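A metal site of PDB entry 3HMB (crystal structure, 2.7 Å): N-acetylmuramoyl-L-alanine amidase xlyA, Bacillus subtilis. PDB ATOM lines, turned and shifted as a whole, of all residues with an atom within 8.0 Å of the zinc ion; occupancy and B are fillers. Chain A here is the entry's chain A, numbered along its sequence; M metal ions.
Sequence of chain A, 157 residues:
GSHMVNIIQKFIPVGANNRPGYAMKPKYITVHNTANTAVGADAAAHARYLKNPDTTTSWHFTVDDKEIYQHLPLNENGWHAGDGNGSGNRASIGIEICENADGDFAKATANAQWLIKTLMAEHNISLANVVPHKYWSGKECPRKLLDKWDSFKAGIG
The nearest printed residue that does not touch the zinc ion is His 80 (4.4 Å).
The zinc ion is bound by a ring nitrogen (ND1) of His 32 (2.1 Å). ND1 of His 133 binds the zinc ion (2.3 Å). The zinc ion is bound by SG of Cys 141 (2.4 Å).
The backbone NH (N) of Lys 134 lies within hydrogen-bond range of the backbone carbonyl oxygen (O) of Cys 141. The backbone NH (N) of His 133 lies within hydrogen-bond range of the backbone carbonyl oxygen (O) of Val 31, 3.2 Å away. A ring nitrogen (NE2) of His 133 lies close to the backbone carbonyl oxygen (O) of His 80 (3.4 Å). The backbone NH (N) of His 32 lies within hydrogen-bond range of the backbone carbonyl oxygen (O) of Ile 95 (2.8 Å). The side-chain hydroxyl (OG) of Ser 137 lies within hydrogen-bond range of a ring nitrogen (NE2) of His 133. NE2 of His 133 lies within hydrogen-bond range of O of Ala 81. A ring nitrogen (NE2) of His 32 sits at hydrogen-bond distance from a ring nitrogen (ND1) of His 80 (2.8 Å). SG of Cys 141 lies close to N of Asn 33 (3.5 Å).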
ATOM      1  N   THR A  30      33.045  16.901  18.064  1.00  0.00           N
ATOM      2  CA  THR A  30      32.160  17.623  17.155  1.00  0.00           C
ATOM      3  C   THR A  30      30.834  18.026  17.789  1.00  0.00           C
ATOM      4  O   THR A  30      30.080  17.188  18.282  1.00  0.00           O
ATOM      5  CB  THR A  30      31.855  16.761  15.901  1.00  0.00           C
ATOM      6  OG1 THR A  30      33.072  16.308  15.313  1.00  0.00           O
ATOM      7  CG2 THR A  30      31.066  17.583  14.884  1.00  0.00           C
ATOM      8  N   VAL A  31      30.547  19.329  17.767  1.00  0.00           N
ATOM      9  CA  VAL A  31      29.313  19.856  18.329  1.00  0.00           C
ATOM     10  C   VAL A  31      28.213  19.980  17.266  1.00  0.00           C
ATOM     11  O   VAL A  31      28.448  20.481  16.167  1.00  0.00           O
ATOM     12  CB  VAL A  31      29.596  21.214  18.997  1.00  0.00           C
ATOM     13  CG1 VAL A  31      28.309  21.866  19.467  1.00  0.00           C
ATOM     14  CG2 VAL A  31      30.542  21.010  20.181  1.00  0.00           C
ATOM     15  N   HIS A  32      27.014  19.526  17.611  1.00  0.00           N
ATOM     16  CA  HIS A  32      25.843  19.540  16.717  1.00  0.00           C
ATOM     17  C   HIS A  32      24.609  20.164  17.393  1.00  0.00           C
ATOM     18  O   HIS A  32      24.556  20.345  18.611  1.00  0.00           O
ATOM     19  CB  HIS A  32      25.438  18.105  16.378  1.00  0.00           C
ATOM     20  CG  HIS A  32      26.452  17.322  15.612  1.00  0.00           C
ATOM     21  ND1 HIS A  32      26.509  17.336  14.229  1.00  0.00           N
ATOM     22  CD2 HIS A  32      27.374  16.423  16.010  1.00  0.00           C
ATOM     23  CE1 HIS A  32      27.414  16.460  13.822  1.00  0.00           C
ATOM     24  NE2 HIS A  32      27.957  15.901  14.880  1.00  0.00           N
ATOM     25  N   ASN A  33      23.600  20.451  16.566  1.00  0.00           N
ATOM     26  CA  ASN A  33      22.319  20.973  17.040  1.00  0.00           C
ATOM     27  C   ASN A  33      21.262  20.147  16.332  1.00  0.00           C
ATOM     28  O   ASN A  33      21.176  20.177  15.110  1.00  0.00           O
ATOM     29  CB  ASN A  33      22.142  22.460  16.693  1.00  0.00           C
ATOM     30  CG  ASN A  33      22.793  23.363  17.737  1.00  0.00           C
ATOM     31  OD1 ASN A  33      23.092  22.914  18.847  1.00  0.00           O
ATOM     32  ND2 ASN A  33      22.988  24.641  17.395  1.00  0.00           N
ATOM     33  N   THR A  34      20.464  19.405  17.090  1.00  0.00           N
ATOM     34  CA  THR A  34      19.442  18.547  16.494  1.00  0.00           C
ATOM     35  C   THR A  34      18.600  19.226  15.430  1.00  0.00           C
ATOM     36  O   THR A  34      18.161  18.576  14.480  1.00  0.00           O
ATOM     37  CB  THR A  34      18.498  17.992  17.545  1.00  0.00           C
ATOM     38  OG1 THR A  34      17.775  19.074  18.118  1.00  0.00           O
ATOM     39  CG2 THR A  34      19.260  17.262  18.625  1.00  0.00           C
ATOM     40  N   ALA A  35      18.381  20.526  15.590  1.00  0.00           N
ATOM     41  CA  ALA A  35      17.562  21.326  14.671  1.00  0.00           C
ATOM     42  C   ALA A  35      16.110  20.833  14.694  1.00  0.00           C
ATOM     43  O   ALA A  35      15.348  21.051  13.763  1.00  0.00           O
ATOM     44  CB  ALA A  35      18.114  21.246  13.273  1.00  0.00           C
ATOM     45  N   TRP A  59      25.524   9.183  17.051  1.00  0.00           N
ATOM     46  CA  TRP A  59      26.533   9.987  17.751  1.00  0.00           C
ATOM     47  C   TRP A  59      26.657   9.475  19.183  1.00  0.00           C
ATOM     48  O   TRP A  59      25.884   8.620  19.617  1.00  0.00           O
ATOM     49  CB  TRP A  59      26.174  11.474  17.716  1.00  0.00           C
ATOM     50  CG  TRP A  59      24.776  11.770  18.097  1.00  0.00           C
ATOM     51  CD1 TRP A  59      24.299  12.118  19.332  1.00  0.00           C
ATOM     52  CD2 TRP A  59      23.626  11.718  17.234  1.00  0.00           C
ATOM     53  NE1 TRP A  59      22.932  12.279  19.284  1.00  0.00           N
ATOM     54  CE2 TRP A  59      22.497  12.041  18.014  1.00  0.00           C
ATOM     55  CE3 TRP A  59      23.448  11.423  15.878  1.00  0.00           C
ATOM     56  CZ2 TRP A  59      21.209  12.070  17.473  1.00  0.00           C
ATOM     57  CZ3 TRP A  59      22.172  11.456  15.345  1.00  0.00           C
ATOM     58  CH2 TRP A  59      21.068  11.781  16.152  1.00  0.00           C
ATOM     59  N   HIS A  80      27.943  11.129  11.799  1.00  0.00           N
ATOM     60  CA  HIS A  80      27.327  12.407  12.115  1.00  0.00           C
ATOM     61  C   HIS A  80      28.005  13.625  11.484  1.00  0.00           C
ATOM     62  O   HIS A  80      27.345  14.643  11.268  1.00  0.00           O
ATOM     63  CB  HIS A  80      27.315  12.564  13.636  1.00  0.00           C
ATOM     64  CG  HIS A  80      28.678  12.460  14.262  1.00  0.00           C
ATOM     65  ND1 HIS A  80      29.478  13.558  14.490  1.00  0.00           N
ATOM     66  CD2 HIS A  80      29.393  11.374  14.633  1.00  0.00           C
ATOM     67  CE1 HIS A  80      30.639  13.156  14.975  1.00  0.00           C
ATOM     68  NE2 HIS A  80      30.618  11.836  15.067  1.00  0.00           N
ATOM     69  N   ALA A  81      29.296  13.521  11.211  1.00  0.00           N
ATOM     70  CA  ALA A  81      30.060  14.619  10.619  1.00  0.00           C
ATOM     71  C   ALA A  81      29.907  14.703   9.105  1.00  0.00           C
ATOM     72  O   ALA A  81      30.430  15.617   8.456  1.00  0.00           O
ATOM     73  CB  ALA A  81      31.533  14.483  10.980  1.00  0.00           C
ATOM     74  N   GLY A  82      29.173  13.754   8.544  1.00  0.00           N
ATOM     75  CA  GLY A  82      28.930  13.707   7.116  1.00  0.00           C
ATOM     76  C   GLY A  82      30.180  13.858   6.279  1.00  0.00           C
ATOM     77  O   GLY A  82      30.149  14.522   5.236  1.00  0.00           O
ATOM     78  N   ILE A  95      28.524  15.169  19.770  1.00  0.00           N
ATOM     79  CA  ILE A  95      27.589  15.632  20.787  1.00  0.00           C
ATOM     80  C   ILE A  95      26.466  16.431  20.140  1.00  0.00           C
ATOM     81  O   ILE A  95      26.702  17.315  19.315  1.00  0.00           O
ATOM     82  CB  ILE A  95      28.284  16.538  21.800  1.00  0.00           C
ATOM     83  CG1 ILE A  95      29.445  15.772  22.437  1.00  0.00           C
ATOM     84  CG2 ILE A  95      27.296  17.004  22.844  1.00  0.00           C
ATOM     85  CD1 ILE A  95      30.253  16.589  23.404  1.00  0.00           C
ATOM     86  N   GLU A  96      25.226  16.108  20.520  1.00  0.00           N
ATOM     87  CA  GLU A  96      24.056  16.784  19.986  1.00  0.00           C
ATOM     88  C   GLU A  96      23.347  17.570  21.077  1.00  0.00           C
ATOM     89  O   GLU A  96      23.134  17.061  22.176  1.00  0.00           O
ATOM     90  CB  GLU A  96      23.084  15.770  19.381  1.00  0.00           C
ATOM     91  CG  GLU A  96      23.489  15.223  18.024  1.00  0.00           C
ATOM     92  CD  GLU A  96      22.823  15.975  16.863  1.00  0.00           C
ATOM     93  OE1 GLU A  96      22.851  17.230  16.851  1.00  0.00           O
ATOM     94  OE2 GLU A  96      22.281  15.298  15.953  1.00  0.00           O
ATOM     95  N   PRO A 132      32.943  22.523  15.226  1.00  0.00           N
ATOM     96  CA  PRO A 132      31.523  22.362  14.927  1.00  0.00           C
ATOM     97  C   PRO A 132      31.395  21.388  13.770  1.00  0.00           C
ATOM     98  O   PRO A 132      32.382  21.048  13.113  1.00  0.00           O
ATOM     99  CB  PRO A 132      31.101  23.767  14.529  1.00  0.00           C
ATOM    100  CG  PRO A 132      32.322  24.289  13.841  1.00  0.00           C
ATOM    101  CD  PRO A 132      33.432  23.841  14.772  1.00  0.00           C
ATOM    102  N   HIS A 133      30.193  20.918  13.525  1.00  0.00           N
ATOM    103  CA  HIS A 133      29.968  19.987  12.430  1.00  0.00           C
ATOM    104  C   HIS A 133      30.421  20.638  11.126  1.00  0.00           C
ATOM    105  O   HIS A 133      31.036  19.991  10.273  1.00  0.00           O
ATOM    106  CB  HIS A 133      28.484  19.604  12.375  1.00  0.00           C
ATOM    107  CG  HIS A 133      28.129  18.699  11.238  1.00  0.00           C
ATOM    108  ND1 HIS A 133      26.834  18.319  10.982  1.00  0.00           N
ATOM    109  CD2 HIS A 133      28.885  18.135  10.268  1.00  0.00           C
ATOM    110  CE1 HIS A 133      26.806  17.563   9.894  1.00  0.00           C
ATOM    111  NE2 HIS A 133      28.037  17.435   9.440  1.00  0.00           N
ATOM    112  N   LYS A 134      30.137  21.940  10.977  1.00  0.00           N
ATOM    113  CA  LYS A 134      30.489  22.695   9.764  1.00  0.00           C
ATOM    114  C   LYS A 134      31.968  22.586   9.403  1.00  0.00           C
ATOM    115  O   LYS A 134      32.343  22.791   8.255  1.00  0.00           O
ATOM    116  CB  LYS A 134      30.118  24.172   9.931  1.00  0.00           C
ATOM    117  CG  LYS A 134      30.089  24.948   8.607  1.00  0.00           C
ATOM    118  CD  LYS A 134      29.754  26.430   8.785  1.00  0.00           C
ATOM    119  CE  LYS A 134      29.560  27.119   7.423  1.00  0.00           C
ATOM    120  NZ  LYS A 134      29.335  28.598   7.538  1.00  0.00           N
ATOM    121  N   SER A 137      31.903  18.983   7.121  1.00  0.00           N
ATOM    122  CA  SER A 137      31.104  18.917   5.906  1.00  0.00           C
ATOM    123  C   SER A 137      30.693  20.283   5.347  1.00  0.00           C
ATOM    124  O   SER A 137      30.222  20.378   4.216  1.00  0.00           O
ATOM    125  CB  SER A 137      29.848  18.061   6.129  1.00  0.00           C
ATOM    126  OG  SER A 137      28.939  18.713   7.004  1.00  0.00           O
ATOM    127  N   LYS A 139      28.326  22.123   6.525  1.00  0.00           N
ATOM    128  CA  LYS A 139      26.892  22.294   6.755  1.00  0.00           C
ATOM    129  C   LYS A 139      26.652  23.308   7.893  1.00  0.00           C
ATOM    130  O   LYS A 139      27.467  23.407   8.806  1.00  0.00           O
ATOM    131  CB  LYS A 139      26.267  20.944   7.111  1.00  0.00           C
ATOM    132  CG  LYS A 139      24.798  21.018   7.462  1.00  0.00           C
ATOM    133  CD  LYS A 139      24.221  19.666   7.895  1.00  0.00           C
ATOM    134  CE  LYS A 139      22.705  19.781   8.093  1.00  0.00           C
ATOM    135  NZ  LYS A 139      22.086  18.513   8.532  1.00  0.00           N
ATOM    136  N   GLU A 140      25.550  24.041   7.851  1.00  0.00           N
ATOM    137  CA  GLU A 140      25.254  25.018   8.906  1.00  0.00           C
ATOM    138  C   GLU A 140      24.841  24.356  10.221  1.00  0.00           C
ATOM    139  O   GLU A 140      23.661  24.367  10.588  1.00  0.00           O
ATOM    140  CB  GLU A 140      24.150  25.992   8.452  1.00  0.00           C
ATOM    141  CG  GLU A 140      24.637  27.121   7.568  1.00  0.00           C
ATOM    142  CD  GLU A 140      25.651  28.006   8.256  1.00  0.00           C
ATOM    143  OE1 GLU A 140      26.779  27.532   8.504  1.00  0.00           O
ATOM    144  OE2 GLU A 140      25.335  29.178   8.568  1.00  0.00           O
ATOM    145  N   CYS A 141      25.821  23.801  10.934  1.00  0.00           N
ATOM    146  CA  CYS A 141      25.573  23.118  12.205  1.00  0.00           C
ATOM    147  C   CYS A 141      26.783  23.253  13.149  1.00  0.00           C
ATOM    148  O   CYS A 141      27.913  23.081  12.712  1.00  0.00           O
ATOM    149  CB  CYS A 141      25.303  21.636  11.897  1.00  0.00           C
ATOM    150  SG  CYS A 141      24.942  20.584  13.310  1.00  0.00           S
ATOM    151  N   PRO A 142      26.576  23.615  14.431  1.00  0.00           N
ATOM    152  CA  PRO A 142      25.336  23.910  15.166  1.00  0.00           C
ATOM    153  C   PRO A 142      24.781  25.277  14.778  1.00  0.00           C
ATOM    154  O   PRO A 142      25.414  26.304  14.991  1.00  0.00           O
ATOM    155  CB  PRO A 142      25.784  23.856  16.626  1.00  0.00           C
ATOM    156  CG  PRO A 142      27.184  24.375  16.562  1.00  0.00           C
ATOM    157  CD  PRO A 142      27.737  23.681  15.338  1.00  0.00           C
ATOM    158  N   ARG A 143      23.575  25.291  14.214  1.00  0.00           N
ATOM    159  CA  ARG A 143      22.962  26.525  13.755  1.00  0.00           C
ATOM    160  C   ARG A 143      22.819  27.654  14.776  1.00  0.00           C
ATOM    161  O   ARG A 143      23.152  28.798  14.480  1.00  0.00           O
ATOM    162  CB  ARG A 143      21.591  26.237  13.145  1.00  0.00           C
ATOM    163  CG  ARG A 143      20.616  25.567  14.072  1.00  0.00           C
ATOM    164  CD  ARG A 143      19.249  25.514  13.441  1.00  0.00           C
ATOM    165  NE  ARG A 143      18.230  24.994  14.357  1.00  0.00           N
ATOM    166  CZ  ARG A 143      16.954  24.806  14.025  1.00  0.00           C
ATOM    167  NH1 ARG A 143      16.536  25.093  12.804  1.00  0.00           N
ATOM    168  NH2 ARG A 143      16.090  24.329  14.922  1.00  0.00           N
HETATM  169 ZN    ZN M   1      25.332  18.299  12.746  1.00  0.00          ZN
